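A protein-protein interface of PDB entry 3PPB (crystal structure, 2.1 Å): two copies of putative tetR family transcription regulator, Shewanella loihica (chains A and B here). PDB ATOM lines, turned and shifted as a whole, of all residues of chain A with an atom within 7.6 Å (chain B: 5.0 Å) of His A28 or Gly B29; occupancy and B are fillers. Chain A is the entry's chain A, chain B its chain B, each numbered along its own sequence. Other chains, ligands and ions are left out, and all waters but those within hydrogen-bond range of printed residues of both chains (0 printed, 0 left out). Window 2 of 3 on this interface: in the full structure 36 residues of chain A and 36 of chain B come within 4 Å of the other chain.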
ATOM      1  N   PHE A  22      18.487   7.230 -16.762  1.00  0.00           N
ATOM      2  CA  PHE A  22      18.306   5.772 -16.786  1.00  0.00           C
ATOM      3  C   PHE A  22      17.770   5.272 -15.441  1.00  0.00           C
ATOM      4  O   PHE A  22      17.114   4.237 -15.397  1.00  0.00           O
ATOM      5  CB  PHE A  22      19.610   5.034 -17.150  1.00  0.00           C
ATOM      6  CG  PHE A  22      20.090   5.176 -18.577  1.00  0.00           C
ATOM      7  CD1 PHE A  22      19.231   5.617 -19.579  1.00  0.00           C
ATOM      8  CD2 PHE A  22      21.392   4.840 -18.924  1.00  0.00           C
ATOM      9  CE1 PHE A  22      19.669   5.728 -20.897  1.00  0.00           C
ATOM     10  CE2 PHE A  22      21.832   4.946 -20.240  1.00  0.00           C
ATOM     11  CZ  PHE A  22      20.971   5.405 -21.222  1.00  0.00           C
ATOM     12  N   GLN A  25      13.851   7.364 -15.239  1.00  0.00           N
ATOM     13  CA  GLN A  25      12.922   7.057 -16.341  1.00  0.00           C
ATOM     14  C   GLN A  25      13.156   5.711 -17.038  1.00  0.00           C
ATOM     15  O   GLN A  25      12.408   5.373 -17.951  1.00  0.00           O
ATOM     16  CB  GLN A  25      13.022   8.144 -17.410  1.00  0.00           C
ATOM     17  CG  GLN A  25      12.514   9.503 -16.971  1.00  0.00           C
ATOM     18  CD  GLN A  25      12.743  10.575 -18.006  1.00  0.00           C
ATOM     19  OE1 GLN A  25      12.678  11.769 -17.699  1.00  0.00           O
ATOM     20  NE2 GLN A  25      13.008  10.189 -19.254  1.00  0.00           N
ATOM     21  N   GLY A  26      14.213   5.000 -16.674  1.00  0.00           N
ATOM     22  CA  GLY A  26      14.553   3.736 -17.310  1.00  0.00           C
ATOM     23  C   GLY A  26      15.331   3.931 -18.595  1.00  0.00           C
ATOM     24  O   GLY A  26      15.458   5.050 -19.088  1.00  0.00           O
ATOM     25  N   PHE A  27      15.846   2.843 -19.147  1.00  0.00           N
ATOM     26  CA  PHE A  27      16.633   2.847 -20.372  1.00  0.00           C
ATOM     27  C   PHE A  27      15.744   3.104 -21.599  1.00  0.00           C
ATOM     28  O   PHE A  27      16.033   4.014 -22.363  1.00  0.00           O
ATOM     29  CB  PHE A  27      17.413   1.522 -20.509  1.00  0.00           C
ATOM     30  CG  PHE A  27      18.124   1.348 -21.826  1.00  0.00           C
ATOM     31  CD1 PHE A  27      19.337   1.982 -22.065  1.00  0.00           C
ATOM     32  CD2 PHE A  27      17.588   0.541 -22.820  1.00  0.00           C
ATOM     33  CE1 PHE A  27      20.000   1.813 -23.274  1.00  0.00           C
ATOM     34  CE2 PHE A  27      18.235   0.397 -24.045  1.00  0.00           C
ATOM     35  CZ  PHE A  27      19.437   1.036 -24.265  1.00  0.00           C
ATOM     36  N   HIS A  28      14.670   2.312 -21.783  1.00  0.00           N
ATOM     37  CA  HIS A  28      13.768   2.453 -22.928  1.00  0.00           C
ATOM     38  C   HIS A  28      12.808   3.632 -22.764  1.00  0.00           C
ATOM     39  O   HIS A  28      12.237   4.085 -23.760  1.00  0.00           O
ATOM     40  CB  HIS A  28      12.977   1.169 -23.169  1.00  0.00           C
ATOM     41  CG  HIS A  28      13.817  -0.036 -23.455  1.00  0.00           C
ATOM     42  ND1 HIS A  28      14.538  -0.153 -24.634  1.00  0.00           N
ATOM     43  CD2 HIS A  28      13.980  -1.161 -22.728  1.00  0.00           C
ATOM     44  CE1 HIS A  28      15.133  -1.332 -24.568  1.00  0.00           C
ATOM     45  NE2 HIS A  28      14.831  -1.971 -23.437  1.00  0.00           N
ATOM     46  N   GLY A  29      12.650   4.120 -21.528  1.00  0.00           N
ATOM     47  CA  GLY A  29      11.824   5.285 -21.220  1.00  0.00           C
ATOM     48  C   GLY A  29      12.552   6.597 -21.464  1.00  0.00           C
ATOM     49  O   GLY A  29      11.948   7.674 -21.408  1.00  0.00           O
ATOM     50  N   THR A  30      13.861   6.513 -21.743  1.00  0.00           N
ATOM     51  CA  THR A  30      14.723   7.670 -21.986  1.00  0.00           C
ATOM     52  C   THR A  30      15.170   7.728 -23.443  1.00  0.00           C
ATOM     53  O   THR A  30      15.731   6.761 -23.947  1.00  0.00           O
ATOM     54  CB  THR A  30      15.947   7.600 -21.057  1.00  0.00           C
ATOM     55  OG1 THR A  30      15.500   7.640 -19.707  1.00  0.00           O
ATOM     56  CG2 THR A  30      16.951   8.721 -21.299  1.00  0.00           C
ATOM     57  N   SER A  31      14.969   8.873 -24.100  1.00  0.00           N
ATOM     58  CA  SER A  31      15.433   9.037 -25.465  1.00  0.00           C
ATOM     59  C   SER A  31      16.811   9.708 -25.459  1.00  0.00           C
ATOM     60  O   SER A  31      17.121  10.466 -24.530  1.00  0.00           O
ATOM     61  CB  SER A  31      14.428   9.853 -26.284  1.00  0.00           C
ATOM     62  OG  SER A  31      14.565  11.248 -26.062  1.00  0.00           O
ATOM     63  N   LYS A  53      22.379   4.018 -27.892  1.00  0.00           N
ATOM     64  CA  LYS A  53      21.961   4.215 -26.506  1.00  0.00           C
ATOM     65  C   LYS A  53      22.434   3.021 -25.671  1.00  0.00           C
ATOM     66  O   LYS A  53      22.768   3.188 -24.501  1.00  0.00           O
ATOM     67  CB  LYS A  53      20.448   4.388 -26.440  1.00  0.00           C
ATOM     68  CG  LYS A  53      19.965   5.090 -25.177  1.00  0.00           C
ATOM     69  CD  LYS A  53      18.463   5.360 -25.224  1.00  0.00           C
ATOM     70  CE  LYS A  53      17.628   4.097 -25.182  1.00  0.00           C
ATOM     71  NZ  LYS A  53      16.184   4.406 -25.181  1.00  0.00           N
ATOM     72  N   GLU A  54      22.498   1.830 -26.312  1.00  0.00           N
ATOM     73  CA  GLU A  54      22.988   0.566 -25.774  1.00  0.00           C
ATOM     74  C   GLU A  54      24.461   0.707 -25.360  1.00  0.00           C
ATOM     75  O   GLU A  54      24.806   0.334 -24.238  1.00  0.00           O
ATOM     76  CB  GLU A  54      22.831  -0.553 -26.823  1.00  0.00           C
ATOM     77  CG  GLU A  54      21.411  -1.070 -27.017  1.00  0.00           C
ATOM     78  CD  GLU A  54      20.420  -0.184 -27.748  1.00  0.00           C
ATOM     79  OE1 GLU A  54      20.847   0.740 -28.477  1.00  0.00           O
ATOM     80  OE2 GLU A  54      19.202  -0.430 -27.600  1.00  0.00           O
ATOM     81  N   LEU A  57      24.767   2.968 -22.300  1.00  0.00           N
ATOM     82  CA  LEU A  57      24.424   2.210 -21.089  1.00  0.00           C
ATOM     83  C   LEU A  57      25.583   1.279 -20.679  1.00  0.00           C
ATOM     84  O   LEU A  57      25.891   1.180 -19.495  1.00  0.00           O
ATOM     85  CB  LEU A  57      23.123   1.387 -21.266  1.00  0.00           C
ATOM     86  CG  LEU A  57      22.785   0.408 -20.112  1.00  0.00           C
ATOM     87  CD1 LEU A  57      22.555   1.151 -18.817  1.00  0.00           C
ATOM     88  CD2 LEU A  57      21.607  -0.498 -20.456  1.00  0.00           C
ATOM     89  N   TYR A 110      20.057  -2.343 -12.833  1.00  0.00           N
ATOM     90  CA  TYR A 110      20.708  -2.929 -14.012  1.00  0.00           C
ATOM     91  C   TYR A 110      21.729  -4.068 -13.794  1.00  0.00           C
ATOM     92  O   TYR A 110      21.953  -4.825 -14.742  1.00  0.00           O
ATOM     93  CB  TYR A 110      21.413  -1.806 -14.808  1.00  0.00           C
ATOM     94  CG  TYR A 110      20.451  -0.765 -15.343  1.00  0.00           C
ATOM     95  CD1 TYR A 110      19.817  -0.938 -16.568  1.00  0.00           C
ATOM     96  CD2 TYR A 110      20.191   0.405 -14.637  1.00  0.00           C
ATOM     97  CE1 TYR A 110      18.912   0.005 -17.054  1.00  0.00           C
ATOM     98  CE2 TYR A 110      19.287   1.353 -15.116  1.00  0.00           C
ATOM     99  CZ  TYR A 110      18.642   1.141 -16.319  1.00  0.00           C
ATOM    100  OH  TYR A 110      17.761   2.071 -16.799  1.00  0.00           O
ATOM    101  N   THR A 115      18.481  -6.483 -18.932  1.00  0.00           N
ATOM    102  CA  THR A 115      18.674  -5.286 -19.772  1.00  0.00           C
ATOM    103  C   THR A 115      20.109  -5.205 -20.326  1.00  0.00           C
ATOM    104  O   THR A 115      20.279  -4.931 -21.522  1.00  0.00           O
ATOM    105  CB  THR A 115      18.304  -3.983 -19.002  1.00  0.00           C
ATOM    106  OG1 THR A 115      17.068  -4.159 -18.313  1.00  0.00           O
ATOM    107  CG2 THR A 115      18.198  -2.770 -19.909  1.00  0.00           C
ATOM    108  N   SER B  24       9.931  -6.387 -22.273  1.00  0.00           N
ATOM    109  CA  SER B  24      10.703  -6.081 -23.474  1.00  0.00           C
ATOM    110  C   SER B  24      10.997  -4.586 -23.676  1.00  0.00           C
ATOM    111  O   SER B  24      12.027  -4.263 -24.267  1.00  0.00           O
ATOM    112  CB  SER B  24      10.009  -6.628 -24.715  1.00  0.00           C
ATOM    113  OG  SER B  24       8.655  -6.217 -24.779  1.00  0.00           O
ATOM    114  N   GLN B  25      10.131  -3.683 -23.193  1.00  0.00           N
ATOM    115  CA  GLN B  25      10.292  -2.231 -23.423  1.00  0.00           C
ATOM    116  C   GLN B  25      10.344  -1.386 -22.159  1.00  0.00           C
ATOM    117  O   GLN B  25      10.486  -0.172 -22.265  1.00  0.00           O
ATOM    118  CB  GLN B  25       9.126  -1.698 -24.270  1.00  0.00           C
ATOM    119  CG  GLN B  25       9.081  -2.203 -25.677  1.00  0.00           C
ATOM    120  CD  GLN B  25       7.840  -1.747 -26.423  1.00  0.00           C
ATOM    121  OE1 GLN B  25       7.500  -2.301 -27.466  1.00  0.00           O
ATOM    122  NE2 GLN B  25       7.131  -0.729 -25.931  1.00  0.00           N
ATOM    123  N   GLY B  26      10.146  -1.994 -21.003  1.00  0.00           N
ATOM    124  CA  GLY B  26      10.137  -1.279 -19.734  1.00  0.00           C
ATOM    125  C   GLY B  26       8.802  -0.651 -19.438  1.00  0.00           C
ATOM    126  O   GLY B  26       7.919  -0.613 -20.299  1.00  0.00           O
ATOM    127  N   PHE B  27       8.652  -0.139 -18.224  1.00  0.00           N
ATOM    128  CA  PHE B  27       7.423   0.495 -17.763  1.00  0.00           C
ATOM    129  C   PHE B  27       7.229   1.876 -18.424  1.00  0.00           C
ATOM    130  O   PHE B  27       6.175   2.123 -19.020  1.00  0.00           O
ATOM    131  CB  PHE B  27       7.432   0.606 -16.217  1.00  0.00           C
ATOM    132  CG  PHE B  27       6.278   1.407 -15.659  1.00  0.00           C
ATOM    133  CD1 PHE B  27       5.012   0.841 -15.533  1.00  0.00           C
ATOM    134  CD2 PHE B  27       6.458   2.725 -15.248  1.00  0.00           C
ATOM    135  CE1 PHE B  27       3.951   1.575 -14.996  1.00  0.00           C
ATOM    136  CE2 PHE B  27       5.384   3.475 -14.751  1.00  0.00           C
ATOM    137  CZ  PHE B  27       4.138   2.895 -14.629  1.00  0.00           C
ATOM    138  N   HIS B  28       8.242   2.759 -18.329  1.00  0.00           N
ATOM    139  CA  HIS B  28       8.169   4.108 -18.899  1.00  0.00           C
ATOM    140  C   HIS B  28       8.365   4.115 -20.418  1.00  0.00           C
ATOM    141  O   HIS B  28       8.002   5.097 -21.069  1.00  0.00           O
ATOM    142  CB  HIS B  28       9.181   5.047 -18.238  1.00  0.00           C
ATOM    143  CG  HIS B  28       8.985   5.218 -16.763  1.00  0.00           C
ATOM    144  ND1 HIS B  28       7.883   5.889 -16.251  1.00  0.00           N
ATOM    145  CD2 HIS B  28       9.793   4.862 -15.740  1.00  0.00           C
ATOM    146  CE1 HIS B  28       8.038   5.880 -14.935  1.00  0.00           C
ATOM    147  NE2 HIS B  28       9.174   5.279 -14.581  1.00  0.00           N
ATOM    148  N   GLY B  29       8.920   3.030 -20.960  1.00  0.00           N
ATOM    149  CA  GLY B  29       9.123   2.861 -22.392  1.00  0.00           C
ATOM    150  C   GLY B  29       7.879   2.348 -23.099  1.00  0.00           C
ATOM    151  O   GLY B  29       7.837   2.291 -24.337  1.00  0.00           O
ATOM    152  N   THR B  30       6.855   1.975 -22.317  1.00  0.00           N
ATOM    153  CA  THR B  30       5.586   1.436 -22.825  1.00  0.00           C
ATOM    154  C   THR B  30       4.445   2.419 -22.588  1.00  0.00           C
ATOM    155  O   THR B  30       4.232   2.844 -21.455  1.00  0.00           O
ATOM    156  CB  THR B  30       5.303   0.085 -22.118  1.00  0.00           C
ATOM    157  OG1 THR B  30       6.352  -0.823 -22.434  1.00  0.00           O
ATOM    158  CG2 THR B  30       3.963  -0.509 -22.493  1.00  0.00           C
ATOM    159  N   SER B  31       3.670   2.732 -23.631  1.00  0.00           N
ATOM    160  CA  SER B  31       2.505   3.609 -23.460  1.00  0.00           C
ATOM    161  C   SER B  31       1.232   2.775 -23.255  1.00  0.00           C
ATOM    162  O   SER B  31       1.154   1.644 -23.737  1.00  0.00           O
ATOM    163  CB  SER B  31       2.330   4.540 -24.657  1.00  0.00           C
ATOM    164  OG  SER B  31       1.676   3.894 -25.736  1.00  0.00           O
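Gln A25 touches His B28, and with the chains exchanged His A28 touches Gln B25. His A28 touches Gly B29, and with the chains exchanged Gly A29 touches His B28. Gly B29 touches its own counterpart, Gly A29. Of the 6 pairs that touch across the chains among the printed residues, 5 have their exchanged pair printed and touching as well.
O of Gly A29 sits at hydrogen-bond distance from NE2 of Gln A25, at 3.5 Å. The backbone carbonyl oxygen (O) of Gly B29 is in hydrogen-bond range of the side-chain amide nitrogen (NE2) of Gln B25 (3.5 Å).
Among the printed residues, pairs that only touch across the chains: His A28 with Gln B25 (3.0 Å), Gln A25 with His B28 (3.3 Å), His A28 with Gly B29 (3.6 Å), Gly A29 with Gly B29 (3.7 Å), His A28 with Ser B24 (3.7 Å) and Gly A29 with His B28 (3.7 Å).
Phe A27 touches none of the printed residues of chain B. Of the printed residues of chain B, His A28 touches Ser B24 (3.7 Å), Gln B25 (3.0 Å) and Gly B29 (3.6 Å). Printed residues of chain B within 4 Å of Gly A29: His B28 (3.7 Å) and Gly B29 (3.7 Å). Printed residues of chain A within 4 Å of Gln B25: His A28 (3.0 Å). Printed residues of chain A within 4 Å of His B28: Gln A25 (3.3 Å) and Gly A29 (3.7 Å). Gly B29 touches just these residues of chain A: His A28 (3.6 Å) and Gly A29 (3.7 Å). The nearest residue of chain B that does not touch His A28 is Gly B26 (4.3 Å). The nearest residue of chain A that does not touch Gly B29 is Gln A25 (5.2 Å).
Hydrophobic or aromatic side chains of chain B within 4 Å of the printed part of chain A: His B28.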
